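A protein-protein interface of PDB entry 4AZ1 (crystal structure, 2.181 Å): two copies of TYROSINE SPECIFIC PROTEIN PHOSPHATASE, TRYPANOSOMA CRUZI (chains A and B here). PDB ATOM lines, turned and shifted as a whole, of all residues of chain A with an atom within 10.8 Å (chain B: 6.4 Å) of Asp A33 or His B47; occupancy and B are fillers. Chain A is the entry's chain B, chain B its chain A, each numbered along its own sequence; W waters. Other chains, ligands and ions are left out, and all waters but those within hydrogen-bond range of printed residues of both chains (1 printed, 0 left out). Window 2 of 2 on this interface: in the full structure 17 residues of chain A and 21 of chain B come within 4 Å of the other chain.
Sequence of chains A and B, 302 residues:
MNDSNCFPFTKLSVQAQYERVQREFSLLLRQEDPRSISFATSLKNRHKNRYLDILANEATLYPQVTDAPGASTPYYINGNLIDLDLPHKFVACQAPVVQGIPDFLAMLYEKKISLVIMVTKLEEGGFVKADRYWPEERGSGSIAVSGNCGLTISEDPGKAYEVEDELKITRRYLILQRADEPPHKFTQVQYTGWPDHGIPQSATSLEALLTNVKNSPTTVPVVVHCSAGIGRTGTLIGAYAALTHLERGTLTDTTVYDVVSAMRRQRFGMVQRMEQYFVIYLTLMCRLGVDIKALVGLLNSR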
ATOM      1  N   SER A  26     -20.868  -5.013 -26.158  1.00  0.00           N
ATOM      2  CA  SER A  26     -21.126  -6.070 -27.133  1.00  0.00           C
ATOM      3  C   SER A  26     -20.053  -6.079 -28.210  1.00  0.00           C
ATOM      4  O   SER A  26     -19.714  -7.133 -28.760  1.00  0.00           O
ATOM      5  CB  SER A  26     -22.517  -5.914 -27.753  1.00  0.00           C
ATOM      6  OG  SER A  26     -23.522  -6.242 -26.809  1.00  0.00           O
ATOM      7  N   LEU A  27     -19.510  -4.898 -28.495  1.00  0.00           N
ATOM      8  CA  LEU A  27     -18.349  -4.774 -29.367  1.00  0.00           C
ATOM      9  C   LEU A  27     -17.110  -5.362 -28.696  1.00  0.00           C
ATOM     10  O   LEU A  27     -16.329  -6.085 -29.320  1.00  0.00           O
ATOM     11  CB  LEU A  27     -18.106  -3.303 -29.717  1.00  0.00           C
ATOM     12  CG  LEU A  27     -16.961  -2.986 -30.686  1.00  0.00           C
ATOM     13  CD1 LEU A  27     -17.172  -3.707 -32.002  1.00  0.00           C
ATOM     14  CD2 LEU A  27     -16.829  -1.481 -30.927  1.00  0.00           C
ATOM     15  N   LEU A  28     -16.927  -5.037 -27.422  1.00  0.00           N
ATOM     16  CA  LEU A  28     -15.787  -5.534 -26.668  1.00  0.00           C
ATOM     17  C   LEU A  28     -15.809  -7.064 -26.563  1.00  0.00           C
ATOM     18  O   LEU A  28     -14.753  -7.707 -26.521  1.00  0.00           O
ATOM     19  CB  LEU A  28     -15.768  -4.882 -25.285  1.00  0.00           C
ATOM     20  CG  LEU A  28     -15.361  -3.412 -25.333  1.00  0.00           C
ATOM     21  CD1 LEU A  28     -15.746  -2.665 -24.053  1.00  0.00           C
ATOM     22  CD2 LEU A  28     -13.870  -3.324 -25.579  1.00  0.00           C
ATOM     23  N   LEU A  29     -17.009  -7.645 -26.550  1.00  0.00           N
ATOM     24  CA  LEU A  29     -17.165  -9.088 -26.352  1.00  0.00           C
ATOM     25  C   LEU A  29     -16.560  -9.893 -27.493  1.00  0.00           C
ATOM     26  O   LEU A  29     -16.210 -11.057 -27.320  1.00  0.00           O
ATOM     27  CB  LEU A  29     -18.645  -9.460 -26.173  1.00  0.00           C
ATOM     28  CG  LEU A  29     -19.274  -9.123 -24.818  1.00  0.00           C
ATOM     29  CD1 LEU A  29     -20.775  -9.369 -24.820  1.00  0.00           C
ATOM     30  CD2 LEU A  29     -18.608  -9.943 -23.724  1.00  0.00           C
ATOM     31  N   ARG A  30     -16.417  -9.260 -28.653  1.00  0.00           N
ATOM     32  CA  ARG A  30     -16.015  -9.971 -29.863  1.00  0.00           C
ATOM     33  C   ARG A  30     -14.640  -9.544 -30.380  1.00  0.00           C
ATOM     34  O   ARG A  30     -14.192 -10.004 -31.435  1.00  0.00           O
ATOM     35  CB  ARG A  30     -17.084  -9.796 -30.952  1.00  0.00           C
ATOM     36  CG  ARG A  30     -18.433 -10.405 -30.581  1.00  0.00           C
ATOM     37  CD  ARG A  30     -19.350 -10.562 -31.785  1.00  0.00           C
ATOM     38  NE  ARG A  30     -20.513 -11.391 -31.466  1.00  0.00           N
ATOM     39  CZ  ARG A  30     -20.527 -12.719 -31.542  1.00  0.00           C
ATOM     40  NH1 ARG A  30     -19.440 -13.374 -31.932  1.00  0.00           N
ATOM     41  NH2 ARG A  30     -21.625 -13.396 -31.228  1.00  0.00           N
ATOM     42  N   GLN A  31     -13.972  -8.682 -29.618  1.00  0.00           N
ATOM     43  CA  GLN A  31     -12.683  -8.118 -30.015  1.00  0.00           C
ATOM     44  C   GLN A  31     -11.561  -9.160 -30.164  1.00  0.00           C
ATOM     45  O   GLN A  31     -10.853  -9.187 -31.175  1.00  0.00           O
ATOM     46  CB  GLN A  31     -12.256  -7.048 -29.001  1.00  0.00           C
ATOM     47  CG  GLN A  31     -10.893  -6.424 -29.265  1.00  0.00           C
ATOM     48  CD  GLN A  31     -10.452  -5.514 -28.141  1.00  0.00           C
ATOM     49  OE1 GLN A  31     -10.974  -4.409 -27.981  1.00  0.00           O
ATOM     50  NE2 GLN A  31      -9.485  -5.970 -27.353  1.00  0.00           N
ATOM     51  N   GLU A  32     -11.399 -10.011 -29.162  1.00  0.00           N
ATOM     52  CA  GLU A  32     -10.263 -10.930 -29.145  1.00  0.00           C
ATOM     53  C   GLU A  32     -10.572 -12.286 -29.791  1.00  0.00           C
ATOM     54  O   GLU A  32     -11.597 -12.904 -29.492  1.00  0.00           O
ATOM     55  CB  GLU A  32      -9.784 -11.138 -27.705  1.00  0.00           C
ATOM     56  CG  GLU A  32      -9.318  -9.870 -27.018  1.00  0.00           C
ATOM     57  CD  GLU A  32      -8.054  -9.312 -27.636  1.00  0.00           C
ATOM     58  OE1 GLU A  32      -7.104 -10.091 -27.869  1.00  0.00           O
ATOM     59  OE2 GLU A  32      -8.007  -8.089 -27.890  1.00  0.00           O
ATOM     60  N   ASP A  33      -9.677 -12.743 -30.666  1.00  0.00           N
ATOM     61  CA  ASP A  33      -9.812 -14.039 -31.339  1.00  0.00           C
ATOM     62  C   ASP A  33      -8.892 -15.063 -30.672  1.00  0.00           C
ATOM     63  O   ASP A  33      -7.684 -15.070 -30.921  1.00  0.00           O
ATOM     64  CB  ASP A  33      -9.473 -13.885 -32.824  1.00  0.00           C
ATOM     65  CG  ASP A  33      -9.503 -15.207 -33.583  1.00  0.00           C
ATOM     66  OD1 ASP A  33      -9.888 -16.246 -32.993  1.00  0.00           O
ATOM     67  OD2 ASP A  33      -9.142 -15.195 -34.777  1.00  0.00           O
ATOM     68  N   PRO A  34      -9.461 -15.931 -29.812  1.00  0.00           N
ATOM     69  CA  PRO A  34      -8.669 -16.906 -29.045  1.00  0.00           C
ATOM     70  C   PRO A  34      -7.930 -17.900 -29.955  1.00  0.00           C
ATOM     71  O   PRO A  34      -6.903 -18.452 -29.564  1.00  0.00           O
ATOM     72  CB  PRO A  34      -9.724 -17.625 -28.187  1.00  0.00           C
ATOM     73  CG  PRO A  34     -11.012 -17.469 -28.947  1.00  0.00           C
ATOM     74  CD  PRO A  34     -10.912 -16.097 -29.594  1.00  0.00           C
ATOM     75  N   ARG A  35      -8.444 -18.098 -31.163  1.00  0.00           N
ATOM     76  CA  ARG A  35      -7.801 -18.954 -32.152  1.00  0.00           C
ATOM     77  C   ARG A  35      -6.427 -18.391 -32.546  1.00  0.00           C
ATOM     78  O   ARG A  35      -5.518 -19.139 -32.904  1.00  0.00           O
ATOM     79  CB  ARG A  35      -8.715 -19.089 -33.380  1.00  0.00           C
ATOM     80  CG  ARG A  35      -8.386 -20.227 -34.341  1.00  0.00           C
ATOM     81  CD  ARG A  35      -9.425 -20.315 -35.468  1.00  0.00           C
ATOM     82  NE  ARG A  35      -9.289 -21.530 -36.276  1.00  0.00           N
ATOM     83  CZ  ARG A  35     -10.141 -22.555 -36.256  1.00  0.00           C
ATOM     84  NH1 ARG A  35     -11.214 -22.522 -35.470  1.00  0.00           N
ATOM     85  NH2 ARG A  35      -9.925 -23.618 -37.028  1.00  0.00           N
ATOM     86  N   SER A  36      -6.276 -17.072 -32.471  1.00  0.00           N
ATOM     87  CA  SER A  36      -5.013 -16.424 -32.825  1.00  0.00           C
ATOM     88  C   SER A  36      -4.161 -16.030 -31.600  1.00  0.00           C
ATOM     89  O   SER A  36      -3.212 -15.255 -31.728  1.00  0.00           O
ATOM     90  CB  SER A  36      -5.271 -15.183 -33.685  1.00  0.00           C
ATOM     91  OG  SER A  36      -5.488 -14.040 -32.868  1.00  0.00           O
ATOM     92  N   ILE A  37      -4.504 -16.551 -30.423  1.00  0.00           N
ATOM     93  CA  ILE A  37      -3.769 -16.228 -29.197  1.00  0.00           C
ATOM     94  C   ILE A  37      -3.078 -17.462 -28.610  1.00  0.00           C
ATOM     95  O   ILE A  37      -3.697 -18.524 -28.497  1.00  0.00           O
ATOM     96  CB  ILE A  37      -4.714 -15.656 -28.119  1.00  0.00           C
ATOM     97  CG1 ILE A  37      -5.304 -14.312 -28.582  1.00  0.00           C
ATOM     98  CG2 ILE A  37      -3.987 -15.498 -26.775  1.00  0.00           C
ATOM     99  CD1 ILE A  37      -6.512 -13.861 -27.764  1.00  0.00           C
ATOM    100  N   SER A  38      -1.810 -17.325 -28.213  1.00  0.00           N
ATOM    101  CA  SER A  38      -1.149 -18.400 -27.459  1.00  0.00           C
ATOM    102  C   SER A  38      -1.505 -18.368 -25.981  1.00  0.00           C
ATOM    103  O   SER A  38      -1.480 -17.317 -25.338  1.00  0.00           O
ATOM    104  CB  SER A  38       0.375 -18.357 -27.606  1.00  0.00           C
ATOM    105  OG  SER A  38       0.970 -19.408 -26.848  1.00  0.00           O
ATOM    106  N   PHE A  39      -1.841 -19.529 -25.443  1.00  0.00           N
ATOM    107  CA  PHE A  39      -2.062 -19.678 -24.012  1.00  0.00           C
ATOM    108  C   PHE A  39      -1.171 -20.834 -23.549  1.00  0.00           C
ATOM    109  O   PHE A  39      -1.508 -21.552 -22.603  1.00  0.00           O
ATOM    110  CB  PHE A  39      -3.529 -20.028 -23.733  1.00  0.00           C
ATOM    111  CG  PHE A  39      -4.507 -18.929 -24.071  1.00  0.00           C
ATOM    112  CD1 PHE A  39      -4.634 -17.817 -23.248  1.00  0.00           C
ATOM    113  CD2 PHE A  39      -5.342 -19.039 -25.182  1.00  0.00           C
ATOM    114  CE1 PHE A  39      -5.549 -16.806 -23.547  1.00  0.00           C
ATOM    115  CE2 PHE A  39      -6.258 -18.038 -25.483  1.00  0.00           C
ATOM    116  CZ  PHE A  39      -6.361 -16.921 -24.666  1.00  0.00           C
ATOM    117  N   ASN A  57      -2.893 -15.163 -21.180  1.00  0.00           N
ATOM    118  CA  ASN A  57      -2.194 -14.970 -22.460  1.00  0.00           C
ATOM    119  C   ASN A  57      -0.683 -15.130 -22.323  1.00  0.00           C
ATOM    120  O   ASN A  57      -0.067 -14.569 -21.403  1.00  0.00           O
ATOM    121  CB  ASN A  57      -2.470 -13.586 -23.071  1.00  0.00           C
ATOM    122  CG  ASN A  57      -3.951 -13.259 -23.168  1.00  0.00           C
ATOM    123  OD1 ASN A  57      -4.709 -13.469 -22.214  1.00  0.00           O
ATOM    124  ND2 ASN A  57      -4.368 -12.725 -24.320  1.00  0.00           N
ATOM    125  N   SER A 261     -10.807  -2.114 -23.868  1.00  0.00           N
ATOM    126  CA  SER A 261     -10.278  -2.704 -25.092  1.00  0.00           C
ATOM    127  C   SER A 261      -8.793  -3.006 -24.910  1.00  0.00           C
ATOM    128  O   SER A 261      -8.324  -4.086 -25.275  1.00  0.00           O
ATOM    129  CB  SER A 261     -10.497  -1.761 -26.277  1.00  0.00           C
ATOM    130  OG  SER A 261      -9.801  -2.213 -27.424  1.00  0.00           O
ATOM    131  N   ARG A 264      -8.381  -6.051 -22.481  1.00  0.00           N
ATOM    132  CA  ARG A 264      -8.720  -7.348 -23.055  1.00  0.00           C
ATOM    133  C   ARG A 264      -7.630  -7.832 -23.989  1.00  0.00           C
ATOM    134  O   ARG A 264      -7.470  -9.029 -24.201  1.00  0.00           O
ATOM    135  CB  ARG A 264     -10.066  -7.296 -23.783  1.00  0.00           C
ATOM    136  CG  ARG A 264     -11.256  -7.243 -22.842  1.00  0.00           C
ATOM    137  CD  ARG A 264     -12.563  -7.587 -23.540  1.00  0.00           C
ATOM    138  NE  ARG A 264     -13.555  -7.973 -22.543  1.00  0.00           N
ATOM    139  CZ  ARG A 264     -14.394  -8.989 -22.678  1.00  0.00           C
ATOM    140  NH1 ARG A 264     -14.375  -9.713 -23.787  1.00  0.00           N
ATOM    141  NH2 ARG A 264     -15.253  -9.277 -21.704  1.00  0.00           N
ATOM    142  N   ARG A 265      -6.875  -6.892 -24.539  1.00  0.00           N
ATOM    143  CA  ARG A 265      -5.781  -7.229 -25.433  1.00  0.00           C
ATOM    144  C   ARG A 265      -4.707  -7.992 -24.653  1.00  0.00           C
ATOM    145  O   ARG A 265      -4.094  -8.935 -25.164  1.00  0.00           O
ATOM    146  CB  ARG A 265      -5.221  -5.936 -26.040  1.00  0.00           C
ATOM    147  CG  ARG A 265      -4.222  -6.118 -27.161  1.00  0.00           C
ATOM    148  CD  ARG A 265      -3.844  -4.767 -27.776  1.00  0.00           C
ATOM    149  NE  ARG A 265      -3.409  -3.801 -26.765  1.00  0.00           N
ATOM    150  CZ  ARG A 265      -2.195  -3.779 -26.215  1.00  0.00           C
ATOM    151  NH1 ARG A 265      -1.281  -4.677 -26.570  1.00  0.00           N
ATOM    152  NH2 ARG A 265      -1.894  -2.861 -25.305  1.00  0.00           N
ATOM    153  N   GLN A 266      -4.526  -7.607 -23.392  1.00  0.00           N
ATOM    154  CA  GLN A 266      -3.422  -8.095 -22.579  1.00  0.00           C
ATOM    155  C   GLN A 266      -3.806  -9.238 -21.638  1.00  0.00           C
ATOM    156  O   GLN A 266      -2.937  -9.958 -21.150  1.00  0.00           O
ATOM    157  CB  GLN A 266      -2.807  -6.927 -21.791  1.00  0.00           C
ATOM    158  CG  GLN A 266      -2.278  -5.791 -22.670  1.00  0.00           C
ATOM    159  CD  GLN A 266      -1.916  -4.545 -21.876  1.00  0.00           C
ATOM    160  OE1 GLN A 266      -0.926  -4.517 -21.139  1.00  0.00           O
ATOM    161  NE2 GLN A 266      -2.718  -3.499 -22.033  1.00  0.00           N
ATOM    162  N   ARG A 267      -5.098  -9.389 -21.354  1.00  0.00           N
ATOM    163  CA  ARG A 267      -5.594 -10.587 -20.651  1.00  0.00           C
ATOM    164  C   ARG A 267      -7.015 -10.860 -21.123  1.00  0.00           C
ATOM    165  O   ARG A 267      -7.934 -10.065 -20.893  1.00  0.00           O
ATOM    166  CB  ARG A 267      -5.531 -10.432 -19.124  1.00  0.00           C
ATOM    167  CG  ARG A 267      -6.209 -11.583 -18.308  1.00  0.00           C
ATOM    168  CD  ARG A 267      -5.877 -11.433 -16.820  1.00  0.00           C
ATOM    169  NE  ARG A 267      -6.482 -12.453 -15.958  1.00  0.00           N
ATOM    170  CZ  ARG A 267      -5.927 -13.627 -15.675  1.00  0.00           C
ATOM    171  NH1 ARG A 267      -4.748 -13.941 -16.203  1.00  0.00           N
ATOM    172  NH2 ARG A 267      -6.546 -14.489 -14.862  1.00  0.00           N
ATOM    173  N   PHE A 268      -7.167 -11.983 -21.814  1.00  0.00           N
ATOM    174  CA  PHE A 268      -8.416 -12.361 -22.460  1.00  0.00           C
ATOM    175  C   PHE A 268      -9.600 -12.316 -21.490  1.00  0.00           C
ATOM    176  O   PHE A 268      -9.545 -12.915 -20.414  1.00  0.00           O
ATOM    177  CB  PHE A 268      -8.247 -13.779 -23.026  1.00  0.00           C
ATOM    178  CG  PHE A 268      -9.338 -14.210 -23.967  1.00  0.00           C
ATOM    179  CD1 PHE A 268      -9.305 -13.840 -25.307  1.00  0.00           C
ATOM    180  CD2 PHE A 268     -10.378 -15.021 -23.520  1.00  0.00           C
ATOM    181  CE1 PHE A 268     -10.301 -14.259 -26.190  1.00  0.00           C
ATOM    182  CE2 PHE A 268     -11.383 -15.441 -24.393  1.00  0.00           C
ATOM    183  CZ  PHE A 268     -11.344 -15.054 -25.729  1.00  0.00           C
ATOM    184  N   GLY A 269     -10.654 -11.591 -21.867  1.00  0.00           N
ATOM    185  CA  GLY A 269     -11.911 -11.600 -21.135  1.00  0.00           C
ATOM    186  C   GLY A 269     -12.115 -10.548 -20.042  1.00  0.00           C
ATOM    187  O   GLY A 269     -13.169 -10.545 -19.398  1.00  0.00           O
ATOM    188  N   LEU B  43     -22.047 -18.683 -37.985  1.00  0.00           N
ATOM    189  CA  LEU B  43     -21.010 -17.900 -38.659  1.00  0.00           C
ATOM    190  C   LEU B  43     -20.483 -16.702 -37.860  1.00  0.00           C
ATOM    191  O   LEU B  43     -19.302 -16.364 -37.955  1.00  0.00           O
ATOM    192  CB  LEU B  43     -21.496 -17.429 -40.032  1.00  0.00           C
ATOM    193  CG  LEU B  43     -21.008 -18.281 -41.203  1.00  0.00           C
ATOM    194  CD1 LEU B  43     -21.733 -17.928 -42.502  1.00  0.00           C
ATOM    195  CD2 LEU B  43     -19.500 -18.142 -41.368  1.00  0.00           C
ATOM    196  N   LYS B  44     -21.344 -16.044 -37.090  1.00  0.00           N
ATOM    197  CA  LYS B  44     -20.861 -14.948 -36.263  1.00  0.00           C
ATOM    198  C   LYS B  44     -20.202 -15.439 -34.972  1.00  0.00           C
ATOM    199  O   LYS B  44     -19.638 -14.647 -34.218  1.00  0.00           O
ATOM    200  CB  LYS B  44     -21.958 -13.903 -35.995  1.00  0.00           C
ATOM    201  CG  LYS B  44     -23.097 -14.359 -35.107  1.00  0.00           C
ATOM    202  CD  LYS B  44     -23.858 -13.157 -34.569  1.00  0.00           C
ATOM    203  CE  LYS B  44     -24.871 -13.565 -33.510  1.00  0.00           C
ATOM    204  NZ  LYS B  44     -25.554 -12.380 -32.919  1.00  0.00           N
ATOM    205  N   ASN B  45     -20.249 -16.746 -34.726  1.00  0.00           N
ATOM    206  CA  ASN B  45     -19.587 -17.304 -33.545  1.00  0.00           C
ATOM    207  C   ASN B  45     -18.371 -18.155 -33.874  1.00  0.00           C
ATOM    208  O   ASN B  45     -18.156 -19.198 -33.252  1.00  0.00           O
ATOM    209  CB  ASN B  45     -20.566 -18.125 -32.699  1.00  0.00           C
ATOM    210  CG  ASN B  45     -21.340 -17.276 -31.723  1.00  0.00           C
ATOM    211  OD1 ASN B  45     -20.802 -16.833 -30.701  1.00  0.00           O
ATOM    212  ND2 ASN B  45     -22.613 -17.047 -32.023  1.00  0.00           N
ATOM    213  N   ARG B  46     -17.564 -17.714 -34.832  1.00  0.00           N
ATOM    214  CA  ARG B  46     -16.417 -18.516 -35.247  1.00  0.00           C
ATOM    215  C   ARG B  46     -15.356 -18.678 -34.159  1.00  0.00           C
ATOM    216  O   ARG B  46     -14.580 -19.635 -34.182  1.00  0.00           O
ATOM    217  CB  ARG B  46     -15.806 -17.988 -36.550  1.00  0.00           C
ATOM    218  CG  ARG B  46     -15.442 -16.521 -36.557  1.00  0.00           C
ATOM    219  CD  ARG B  46     -14.668 -16.204 -37.829  1.00  0.00           C
ATOM    220  NE  ARG B  46     -15.166 -17.003 -38.947  1.00  0.00           N
ATOM    221  CZ  ARG B  46     -14.523 -17.173 -40.098  1.00  0.00           C
ATOM    222  NH1 ARG B  46     -13.344 -16.597 -40.296  1.00  0.00           N
ATOM    223  NH2 ARG B  46     -15.062 -17.924 -41.051  1.00  0.00           N
ATOM    224  N   HIS B  47     -15.338 -17.752 -33.199  1.00  0.00           N
ATOM    225  CA  HIS B  47     -14.436 -17.851 -32.059  1.00  0.00           C
ATOM    226  C   HIS B  47     -14.690 -19.139 -31.291  1.00  0.00           C
ATOM    227  O   HIS B  47     -13.801 -19.642 -30.610  1.00  0.00           O
ATOM    228  CB  HIS B  47     -14.617 -16.662 -31.100  1.00  0.00           C
ATOM    229  CG  HIS B  47     -14.106 -15.355 -31.631  1.00  0.00           C
ATOM    230  ND1 HIS B  47     -13.496 -15.230 -32.861  1.00  0.00           N
ATOM    231  CD2 HIS B  47     -14.117 -14.115 -31.086  1.00  0.00           C
ATOM    232  CE1 HIS B  47     -13.156 -13.966 -33.054  1.00  0.00           C
ATOM    233  NE2 HIS B  47     -13.525 -13.268 -31.997  1.00  0.00           N
ATOM    234  N   LYS B  48     -15.909 -19.665 -31.390  1.00  0.00           N
ATOM    235  CA  LYS B  48     -16.275 -20.859 -30.637  1.00  0.00           C
ATOM    236  C   LYS B  48     -16.455 -22.069 -31.527  1.00  0.00           C
ATOM    237  O   LYS B  48     -16.864 -23.143 -31.071  1.00  0.00           O
ATOM    238  CB  LYS B  48     -17.534 -20.611 -29.799  1.00  0.00           C
ATOM    239  CG  LYS B  48     -17.296 -19.667 -28.627  1.00  0.00           C
ATOM    240  CD  LYS B  48     -18.592 -19.317 -27.918  1.00  0.00           C
ATOM    241  CE  LYS B  48     -18.320 -18.400 -26.723  1.00  0.00           C
ATOM    242  NZ  LYS B  48     -19.580 -17.843 -26.163  1.00  0.00           N
ATOM    243  N   ASN B  49     -16.160 -21.898 -32.808  1.00  0.00           N
ATOM    244  CA  ASN B  49     -16.183 -23.034 -33.716  1.00  0.00           C
ATOM    245  C   ASN B  49     -14.826 -23.729 -33.714  1.00  0.00           C
ATOM    246  O   ASN B  49     -13.789 -23.077 -33.895  1.00  0.00           O
ATOM    247  CB  ASN B  49     -16.575 -22.569 -35.119  1.00  0.00           C
ATOM    248  CG  ASN B  49     -18.022 -22.121 -35.190  1.00  0.00           C
ATOM    249  OD1 ASN B  49     -18.851 -22.559 -34.388  1.00  0.00           O
ATOM    250  ND2 ASN B  49     -18.339 -21.261 -36.154  1.00  0.00           N
ATOM    251  N   ARG B  50     -14.827 -25.040 -33.485  1.00  0.00           N
ATOM    252  CA  ARG B  50     -13.596 -25.811 -33.548  1.00  0.00           C
ATOM    253  C   ARG B  50     -13.033 -25.833 -34.981  1.00  0.00           C
ATOM    254  O   ARG B  50     -11.824 -25.745 -35.194  1.00  0.00           O
ATOM    255  CB  ARG B  50     -13.835 -27.228 -33.037  1.00  0.00           C
ATOM    256  CG  ARG B  50     -12.570 -28.094 -32.953  1.00  0.00           C
ATOM    257  CD  ARG B  50     -12.845 -29.463 -32.289  1.00  0.00           C
ATOM    258  NE  ARG B  50     -13.178 -29.319 -30.867  1.00  0.00           N
ATOM    259  CZ  ARG B  50     -12.281 -29.153 -29.897  1.00  0.00           C
ATOM    260  NH1 ARG B  50     -10.989 -29.129 -30.183  1.00  0.00           N
ATOM    261  NH2 ARG B  50     -12.670 -29.016 -28.631  1.00  0.00           N
ATOM    262  N   LEU B  52     -13.471 -23.988 -38.784  1.00  0.00           N
ATOM    263  CA  LEU B  52     -14.039 -22.834 -39.480  1.00  0.00           C
ATOM    264  C   LEU B  52     -15.179 -23.140 -40.467  1.00  0.00           C
ATOM    265  O   LEU B  52     -16.158 -22.392 -40.527  1.00  0.00           O
ATOM    266  CB  LEU B  52     -12.929 -22.026 -40.160  1.00  0.00           C
ATOM    267  CG  LEU B  52     -12.014 -21.299 -39.165  1.00  0.00           C
ATOM    268  CD1 LEU B  52     -11.070 -20.347 -39.877  1.00  0.00           C
ATOM    269  CD2 LEU B  52     -12.823 -20.565 -38.086  1.00  0.00           C
ATOM    270  N   VAL B  97     -14.842 -26.052 -27.756  1.00  0.00           N
ATOM    271  CA  VAL B  97     -13.489 -25.578 -27.503  1.00  0.00           C
ATOM    272  C   VAL B  97     -13.458 -24.999 -26.092  1.00  0.00           C
ATOM    273  O   VAL B  97     -14.512 -24.785 -25.489  1.00  0.00           O
ATOM    274  CB  VAL B  97     -13.039 -24.536 -28.544  1.00  0.00           C
ATOM    275  CG1 VAL B  97     -13.161 -25.111 -29.956  1.00  0.00           C
ATOM    276  CG2 VAL B  97     -13.860 -23.257 -28.421  1.00  0.00           C
ATOM    277  N   GLN B  99     -12.978 -22.110 -24.709  1.00  0.00           N
ATOM    278  CA  GLN B  99     -13.774 -20.914 -24.452  1.00  0.00           C
ATOM    279  C   GLN B  99     -15.270 -21.141 -24.695  1.00  0.00           C
ATOM    280  O   GLN B  99     -16.095 -20.291 -24.362  1.00  0.00           O
ATOM    281  CB  GLN B  99     -13.255 -19.722 -25.263  1.00  0.00           C
ATOM    282  CG  GLN B  99     -11.760 -19.429 -25.056  1.00  0.00           C
ATOM    283  CD  GLN B  99     -11.389 -19.022 -23.624  1.00  0.00           C
ATOM    284  OE1 GLN B  99     -12.253 -18.769 -22.779  1.00  0.00           O
ATOM    285  NE2 GLN B  99     -10.086 -18.948 -23.357  1.00  0.00           N
ATOM    286  N   GLY B 100     -15.624 -22.300 -25.242  1.00  0.00           N
ATOM    287  CA  GLY B 100     -17.019 -22.624 -25.493  1.00  0.00           C
ATOM    288  C   GLY B 100     -17.572 -23.635 -24.502  1.00  0.00           C
ATOM    289  O   GLY B 100     -18.771 -23.931 -24.502  1.00  0.00           O
HETATM  290  O   HOH W   1     -10.560 -25.027 -39.590  1.00  0.00           O
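The guanidinium group (NH1) of Arg A30 lies within hydrogen-bond range of the backbone carbonyl oxygen (O) of Lys B44 (2.6 Å).
The backbone carbonyl oxygen (O) of Arg A30 is in hydrogen-bond range of a ring nitrogen (NE2) of His B47 (3.4 Å).
A ring nitrogen (NE2) of His B47 lies within hydrogen-bond range of the backbone carbonyl oxygen of Glu A32 (3.2 Å).
The backbone carbonyl oxygen of Asn B49 lies within hydrogen-bond range of the guanidinium group of Arg A35 (3.1 Å).
O of Arg B50 sits at hydrogen-bond distance from NH1 of Arg A35 (3.3 Å).
NE2 of Gln A31 lies within hydrogen-bond range of OE2 of Glu A32 (2.6 Å).
The backbone NH of Arg A35 lies within hydrogen-bond range of the side-chain carboxylate of Asp A33, at 3.0 Å.
OG of Ser A36 is in hydrogen-bond range of O of Asp A33, at 3.1 Å.
The backbone NH of Phe A268 sits at hydrogen-bond distance from the side-chain amide oxygen of Asn A57 (2.9 Å).
Among the printed residues, merely in contact across the chains: Arg A30 with Asn B45, Arg A35 with Leu B52, Phe A268 with Gln B99, Asp A33 with His B47 and Pro A34 with His B47.
Printed residues of chain B within 4 Å of Glu A32: His B47.
Asp A33 touches just one residue of chain B: His B47.
Printed residues of chain B within 4 Å of Arg A35: Asn B49, Arg B50 and Leu B52.
Printed residues of chain A within 4 Å of Asn B45: Arg A30 (3.6 Å).
Printed residues of chain A within 4 Å of His B47: Arg A30, Glu A32, Asp A33 and Pro A34.
Of chain A, only Arg A35 comes within 4 Å of Asn B49.
Printed residues of chain A within 4 Å of Gln B99: Phe A268 (3.7 Å).
The nearest residue of chain B that does not touch Asp A33 is Arg B46 (5.9 Å).
The nearest printed residue of chain B that does not touch Phe A268 is His B47 (6.1 Å).
Printed residues of chain B that touch a printed residue of chain A: Lys B44, Asn B45, His B47, Asn B49, Arg B50, Leu B52 and Gln B99.
Hydrophobic or aromatic side chains of chain B that line the printed part of chain A: His B47 and Leu B52.
Along chain B the printed residues that touch a printed residue of chain A span positions 44 to 99.
Hydrophobic or aromatic side chains of chain A within 4 Å of the printed part of chain B: Pro A34 and Phe A268.
No position is printed for both chains.
Water W1 lies within hydrogen-bond range of NH2 of Arg A35 and N of Leu B52.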
